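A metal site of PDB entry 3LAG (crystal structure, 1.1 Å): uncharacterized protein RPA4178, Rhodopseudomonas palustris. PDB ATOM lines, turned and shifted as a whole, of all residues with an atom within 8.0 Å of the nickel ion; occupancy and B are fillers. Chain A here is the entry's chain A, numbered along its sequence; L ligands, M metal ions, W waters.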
ATOM      1  N   TRP A  22     -13.785  -1.857  17.120  1.00  0.00           N
ATOM      2  CA  TRP A  22     -14.811  -2.664  16.483  1.00  0.00           C
ATOM      3  C   TRP A  22     -16.158  -2.327  17.072  1.00  0.00           C
ATOM      4  O   TRP A  22     -16.318  -2.290  18.297  1.00  0.00           O
ATOM      5  CB  TRP A  22     -14.503  -4.151  16.687  1.00  0.00           C
ATOM      6  CG  TRP A  22     -13.382  -4.624  15.841  1.00  0.00           C
ATOM      7  CD1 TRP A  22     -12.072  -4.766  16.212  1.00  0.00           C
ATOM      8  CD2 TRP A  22     -13.436  -4.987  14.449  1.00  0.00           C
ATOM      9  NE1 TRP A  22     -11.315  -5.206  15.150  1.00  0.00           N
ATOM     10  CE2 TRP A  22     -12.132  -5.344  14.060  1.00  0.00           C
ATOM     11  CE3 TRP A  22     -14.463  -5.048  13.504  1.00  0.00           C
ATOM     12  CZ2 TRP A  22     -11.827  -5.755  12.764  1.00  0.00           C
ATOM     13  CZ3 TRP A  22     -14.164  -5.459  12.220  1.00  0.00           C
ATOM     14  CH2 TRP A  22     -12.856  -5.798  11.856  1.00  0.00           C
ATOM     15  N   THR A  30     -18.519 -10.257  11.854  1.00  0.00           N
ATOM     16  CA  THR A  30     -17.233  -9.961  11.258  1.00  0.00           C
ATOM     17  C   THR A  30     -17.018 -10.797  10.001  1.00  0.00           C
ATOM     18  O   THR A  30     -16.249 -10.419   9.128  1.00  0.00           O
ATOM     19  CB  THR A  30     -16.066 -10.276  12.239  1.00  0.00           C
ATOM     20  OG1 THR A  30     -16.111 -11.655  12.628  1.00  0.00           O
ATOM     21  CG2 THR A  30     -16.142  -9.385  13.480  1.00  0.00           C
ATOM     22  N   GLY A  31     -17.681 -11.954   9.930  1.00  0.00           N
ATOM     23  CA  GLY A  31     -17.285 -12.982   9.000  1.00  0.00           C
ATOM     24  C   GLY A  31     -16.102 -13.740   9.577  1.00  0.00           C
ATOM     25  O   GLY A  31     -15.347 -13.208  10.408  1.00  0.00           O
ATOM     26  N   HIS A  32     -15.946 -14.988   9.167  1.00  0.00           N
ATOM     27  CA  HIS A  32     -14.779 -15.741   9.578  1.00  0.00           C
ATOM     28  C   HIS A  32     -13.505 -15.019   9.177  1.00  0.00           C
ATOM     29  O   HIS A  32     -13.397 -14.495   8.064  1.00  0.00           O
ATOM     30  CB  HIS A  32     -14.775 -17.141   8.971  1.00  0.00           C
ATOM     31  CG  HIS A  32     -13.621 -17.981   9.429  1.00  0.00           C
ATOM     32  ND1 HIS A  32     -13.720 -18.859  10.484  1.00  0.00           N
ATOM     33  CD2 HIS A  32     -12.336 -18.032   9.004  1.00  0.00           C
ATOM     34  CE1 HIS A  32     -12.547 -19.443  10.667  1.00  0.00           C
ATOM     35  NE2 HIS A  32     -11.697 -18.955   9.787  1.00  0.00           N
ATOM     36  N   HIS A  33     -12.541 -15.004  10.086  1.00  0.00           N
ATOM     37  CA  HIS A  33     -11.244 -14.404   9.798  1.00  0.00           C
ATOM     38  C   HIS A  33     -10.158 -15.082  10.637  1.00  0.00           C
ATOM     39  O   HIS A  33     -10.452 -15.804  11.595  1.00  0.00           O
ATOM     40  CB  HIS A  33     -11.257 -12.913  10.065  1.00  0.00           C
ATOM     41  CG  HIS A  33     -11.633 -12.562  11.464  1.00  0.00           C
ATOM     42  ND1 HIS A  33     -12.943 -12.512  11.885  1.00  0.00           N
ATOM     43  CD2 HIS A  33     -10.872 -12.281  12.542  1.00  0.00           C
ATOM     44  CE1 HIS A  33     -12.970 -12.188  13.164  1.00  0.00           C
ATOM     45  NE2 HIS A  33     -11.733 -12.058  13.591  1.00  0.00           N
ATOM     46  N   THR A  34      -8.917 -14.847  10.243  1.00  0.00           N
ATOM     47  CA  THR A  34      -7.755 -15.463  10.872  1.00  0.00           C
ATOM     48  C   THR A  34      -6.881 -14.397  11.490  1.00  0.00           C
ATOM     49  O   THR A  34      -6.608 -13.353  10.886  1.00  0.00           O
ATOM     50  CB  THR A  34      -6.934 -16.257   9.832  1.00  0.00           C
ATOM     51  OG1 THR A  34      -7.723 -17.340   9.335  1.00  0.00           O
ATOM     52  CG2 THR A  34      -5.666 -16.795  10.459  1.00  0.00           C
ATOM     53  N   HIS A  35      -6.430 -14.639  12.711  1.00  0.00           N
ATOM     54  CA  HIS A  35      -5.538 -13.693  13.369  1.00  0.00           C
ATOM     55  C   HIS A  35      -4.071 -13.948  13.107  1.00  0.00           C
ATOM     56  O   HIS A  35      -3.566 -15.024  13.387  1.00  0.00           O
ATOM     57  CB  HIS A  35      -5.836 -13.636  14.865  1.00  0.00           C
ATOM     58  CG  HIS A  35      -7.064 -12.855  15.175  1.00  0.00           C
ATOM     59  ND1 HIS A  35      -7.041 -11.491  15.390  1.00  0.00           N
ATOM     60  CD2 HIS A  35      -8.363 -13.219  15.244  1.00  0.00           C
ATOM     61  CE1 HIS A  35      -8.262 -11.058  15.601  1.00  0.00           C
ATOM     62  NE2 HIS A  35      -9.083 -12.085  15.524  1.00  0.00           N
ATOM     63  N   TYR A  39      -2.945 -10.633  20.245  1.00  0.00           N
ATOM     64  CA  TYR A  39      -3.740  -9.424  20.438  1.00  0.00           C
ATOM     65  C   TYR A  39      -4.365  -9.360  21.807  1.00  0.00           C
ATOM     66  O   TYR A  39      -4.499 -10.383  22.493  1.00  0.00           O
ATOM     67  CB  TYR A  39      -4.827  -9.293  19.366  1.00  0.00           C
ATOM     68  CG  TYR A  39      -5.887 -10.386  19.289  1.00  0.00           C
ATOM     69  CD1 TYR A  39      -7.139 -10.204  19.855  1.00  0.00           C
ATOM     70  CD2 TYR A  39      -5.647 -11.578  18.601  1.00  0.00           C
ATOM     71  CE1 TYR A  39      -8.126 -11.174  19.767  1.00  0.00           C
ATOM     72  CE2 TYR A  39      -6.632 -12.558  18.498  1.00  0.00           C
ATOM     73  CZ  TYR A  39      -7.867 -12.352  19.086  1.00  0.00           C
ATOM     74  OH  TYR A  39      -8.839 -13.326  18.981  1.00  0.00           O
ATOM     75  N   VAL A  41      -7.818  -7.727  23.738  1.00  0.00           N
ATOM     76  CA  VAL A  41      -9.157  -7.175  23.563  1.00  0.00           C
ATOM     77  C   VAL A  41      -9.523  -6.361  24.796  1.00  0.00           C
ATOM     78  O   VAL A  41      -9.374  -6.838  25.920  1.00  0.00           O
ATOM     79  CB  VAL A  41     -10.199  -8.295  23.379  1.00  0.00           C
ATOM     80  CG1 VAL A  41     -11.615  -7.717  23.330  1.00  0.00           C
ATOM     81  CG2 VAL A  41      -9.888  -9.096  22.134  1.00  0.00           C
ATOM     82  N   MET A  49     -20.997 -11.813  22.974  1.00  0.00           N
ATOM     83  CA  MET A  49     -20.537 -12.106  21.618  1.00  0.00           C
ATOM     84  C   MET A  49     -20.878 -13.565  21.281  1.00  0.00           C
ATOM     85  O   MET A  49     -20.838 -14.433  22.158  1.00  0.00           O
ATOM     86  CB  MET A  49     -19.009 -11.900  21.560  1.00  0.00           C
ATOM     87  CG  MET A  49     -18.462 -10.979  20.459  1.00  0.00           C
ATOM     88  SD  MET A  49     -16.535 -10.473  20.605  1.00  0.00           S
ATOM     89  CE  MET A  49     -15.756 -12.231  20.935  1.00  0.00           C
ATOM     90  N   TYR A  69      -8.530  -9.089  27.844  1.00  0.00           N
ATOM     91  CA  TYR A  69      -8.028 -10.451  27.732  1.00  0.00           C
ATOM     92  C   TYR A  69      -7.099 -10.552  26.543  1.00  0.00           C
ATOM     93  O   TYR A  69      -7.121  -9.720  25.630  1.00  0.00           O
ATOM     94  CB  TYR A  69      -9.176 -11.476  27.656  1.00  0.00           C
ATOM     95  CG  TYR A  69     -10.143 -11.328  26.500  1.00  0.00           C
ATOM     96  CD1 TYR A  69      -9.902 -11.973  25.282  1.00  0.00           C
ATOM     97  CD2 TYR A  69     -11.311 -10.577  26.613  1.00  0.00           C
ATOM     98  CE1 TYR A  69     -10.800 -11.865  24.223  1.00  0.00           C
ATOM     99  CE2 TYR A  69     -12.209 -10.469  25.555  1.00  0.00           C
ATOM    100  CZ  TYR A  69     -11.939 -11.119  24.360  1.00  0.00           C
ATOM    101  OH  TYR A  69     -12.810 -11.020  23.291  1.00  0.00           O
ATOM    102  N   ARG A  71      -5.018 -12.943  23.500  1.00  0.00           N
ATOM    103  CA  ARG A  71      -5.156 -14.037  22.561  1.00  0.00           C
ATOM    104  C   ARG A  71      -3.888 -14.169  21.725  1.00  0.00           C
ATOM    105  O   ARG A  71      -3.133 -13.208  21.601  1.00  0.00           O
ATOM    106  CB  ARG A  71      -6.354 -13.762  21.655  1.00  0.00           C
ATOM    107  CG  ARG A  71      -7.693 -13.771  22.380  1.00  0.00           C
ATOM    108  CD  ARG A  71      -8.016 -15.181  22.779  1.00  0.00           C
ATOM    109  NE  ARG A  71      -9.274 -15.329  23.490  1.00  0.00           N
ATOM    110  CZ  ARG A  71      -9.379 -15.436  24.813  1.00  0.00           C
ATOM    111  NH1 ARG A  71      -8.296 -15.375  25.580  1.00  0.00           N
ATOM    112  NH2 ARG A  71     -10.567 -15.604  25.369  1.00  0.00           N
ATOM    113  N   VAL A  75      -5.735 -17.680  16.006  1.00  0.00           N
ATOM    114  CA  VAL A  75      -7.166 -17.741  16.242  1.00  0.00           C
ATOM    115  C   VAL A  75      -7.926 -17.601  14.926  1.00  0.00           C
ATOM    116  O   VAL A  75      -7.630 -16.707  14.139  1.00  0.00           O
ATOM    117  CB  VAL A  75      -7.638 -16.635  17.225  1.00  0.00           C
ATOM    118  CG1 VAL A  75      -9.172 -16.591  17.303  1.00  0.00           C
ATOM    119  CG2 VAL A  75      -7.044 -16.869  18.610  1.00  0.00           C
ATOM    120  N   GLN A  76      -8.890 -18.486  14.701  1.00  0.00           N
ATOM    121  CA  GLN A  76      -9.764 -18.438  13.525  1.00  0.00           C
ATOM    122  C   GLN A  76     -11.218 -18.531  13.996  1.00  0.00           C
ATOM    123  O   GLN A  76     -11.597 -19.495  14.661  1.00  0.00           O
ATOM    124  CB  GLN A  76      -9.456 -19.590  12.568  1.00  0.00           C
ATOM    125  CG  GLN A  76      -8.084 -19.493  11.908  1.00  0.00           C
ATOM    126  CD  GLN A  76      -7.762 -20.682  11.024  1.00  0.00           C
ATOM    127  OE1 GLN A  76      -8.085 -21.821  11.351  1.00  0.00           O
ATOM    128  NE2 GLN A  76      -7.093 -20.416   9.906  1.00  0.00           N
ATOM    129  N   HIS A  77     -12.022 -17.533  13.656  1.00  0.00           N
ATOM    130  CA  HIS A  77     -13.383 -17.473  14.170  1.00  0.00           C
ATOM    131  C   HIS A  77     -14.225 -16.477  13.380  1.00  0.00           C
ATOM    132  O   HIS A  77     -13.686 -15.647  12.666  1.00  0.00           O
ATOM    133  CB  HIS A  77     -13.395 -17.086  15.663  1.00  0.00           C
ATOM    134  CG  HIS A  77     -12.765 -15.765  15.998  1.00  0.00           C
ATOM    135  ND1 HIS A  77     -12.503 -15.387  17.301  1.00  0.00           N
ATOM    136  CD2 HIS A  77     -12.349 -14.735  15.220  1.00  0.00           C
ATOM    137  CE1 HIS A  77     -11.952 -14.188  17.308  1.00  0.00           C
ATOM    138  NE2 HIS A  77     -11.850 -13.764  16.064  1.00  0.00           N
ATOM    139  N   ASP A  78     -15.536 -16.607  13.521  1.00  0.00           N
ATOM    140  CA  ASP A  78     -16.479 -15.584  13.089  1.00  0.00           C
ATOM    141  C   ASP A  78     -17.093 -15.067  14.364  1.00  0.00           C
ATOM    142  O   ASP A  78     -17.589 -15.843  15.197  1.00  0.00           O
ATOM    143  CB  ASP A  78     -17.546 -16.209  12.177  1.00  0.00           C
ATOM    144  CG  ASP A  78     -18.521 -15.187  11.605  1.00  0.00           C
ATOM    145  OD1 ASP A  78     -18.266 -13.967  11.704  1.00  0.00           O
ATOM    146  OD2 ASP A  78     -19.541 -15.624  11.026  1.00  0.00           O
ATOM    147  N   VAL A  79     -17.063 -13.752  14.521  1.00  0.00           N
ATOM    148  CA  VAL A  79     -17.648 -13.103  15.692  1.00  0.00           C
ATOM    149  C   VAL A  79     -18.926 -12.390  15.261  1.00  0.00           C
ATOM    150  O   VAL A  79     -18.923 -11.557  14.352  1.00  0.00           O
ATOM    151  CB  VAL A  79     -16.658 -12.132  16.348  1.00  0.00           C
ATOM    152  CG1 VAL A  79     -17.351 -11.295  17.415  1.00  0.00           C
ATOM    153  CG2 VAL A  79     -15.472 -12.926  16.936  1.00  0.00           C
ATOM    154  N   PHE A  89     -15.597  -3.030  21.181  1.00  0.00           N
ATOM    155  CA  PHE A  89     -14.336  -3.350  21.822  1.00  0.00           C
ATOM    156  C   PHE A  89     -13.187  -2.818  21.003  1.00  0.00           C
ATOM    157  O   PHE A  89     -13.305  -2.615  19.802  1.00  0.00           O
ATOM    158  CB  PHE A  89     -14.161  -4.871  22.035  1.00  0.00           C
ATOM    159  CG  PHE A  89     -14.261  -5.700  20.776  1.00  0.00           C
ATOM    160  CD1 PHE A  89     -13.117  -6.058  20.059  1.00  0.00           C
ATOM    161  CD2 PHE A  89     -15.490  -6.167  20.326  1.00  0.00           C
ATOM    162  CE1 PHE A  89     -13.218  -6.846  18.907  1.00  0.00           C
ATOM    163  CE2 PHE A  89     -15.585  -6.967  19.169  1.00  0.00           C
ATOM    164  CZ  PHE A  89     -14.449  -7.303  18.471  1.00  0.00           C
ATOM    165  N   GLU A  91      -9.381  -3.780  19.757  1.00  0.00           N
ATOM    166  CA  GLU A  91      -8.472  -4.889  19.534  1.00  0.00           C
ATOM    167  C   GLU A  91      -7.104  -4.311  19.273  1.00  0.00           C
ATOM    168  O   GLU A  91      -6.916  -3.518  18.353  1.00  0.00           O
ATOM    169  CB  GLU A  91      -8.932  -5.714  18.361  1.00  0.00           C
ATOM    170  CG  GLU A  91      -8.400  -7.104  18.383  1.00  0.00           C
ATOM    171  CD  GLU A  91      -9.324  -8.040  17.662  1.00  0.00           C
ATOM    172  OE1 GLU A  91     -10.179  -8.660  18.329  1.00  0.00           O
ATOM    173  OE2 GLU A  91      -9.195  -8.128  16.434  1.00  0.00           O
ATOM    174  N   GLU A  93      -3.530  -5.313  18.310  1.00  0.00           N
ATOM    175  CA  GLU A  93      -2.687  -6.338  17.720  1.00  0.00           C
ATOM    176  C   GLU A  93      -1.224  -6.003  17.961  1.00  0.00           C
ATOM    177  O   GLU A  93      -0.788  -4.868  17.814  1.00  0.00           O
ATOM    178  CB  GLU A  93      -2.967  -6.478  16.235  1.00  0.00           C
ATOM    179  CG  GLU A  93      -4.330  -7.061  15.925  1.00  0.00           C
ATOM    180  CD  GLU A  93      -4.543  -7.175  14.448  1.00  0.00           C
ATOM    181  OE1 GLU A  93      -4.894  -6.149  13.821  1.00  0.00           O
ATOM    182  OE2 GLU A  93      -4.356  -8.276  13.894  1.00  0.00           O
HETATM  183  C1  LIG L   1     -12.059 -10.534  17.186  1.00  0.00           C
HETATM  184  O1  LIG L   1     -12.861 -10.738  16.226  1.00  0.00           O
HETATM  185  O2  LIG L   1     -10.957 -11.074  17.498  1.00  0.00           O
HETATM  186 NI    NI M   1     -11.110 -11.739  15.566  1.00  0.00          NI
HETATM  187  O   HOH W   1     -10.701  -9.379  15.014  1.00  0.00           O
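N of His 35 is in hydrogen-bond range of O of Val 75. A ring nitrogen (ND1) of His 33 lies close to the side-chain hydroxyl (OG1) of Thr 30, 3.4 Å away. ND1 of His 33 lies within hydrogen-bond range of O of Gly 31 (2.9 Å).
Three residues have an atom within 4 Å of the nickel ion: His 33, His 35 and His 77.
The nickel ion is bound by O2 of the ligand (2.0 Å), NE2 of His 35 (2.1 Å), NE2 of His 33 (2.1 Å), O1 of the ligand (2.1 Å), NE2 of His 77 (2.2 Å) and water W1 (2.5 Å). The nickel ion has six donor atoms within binding distance.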
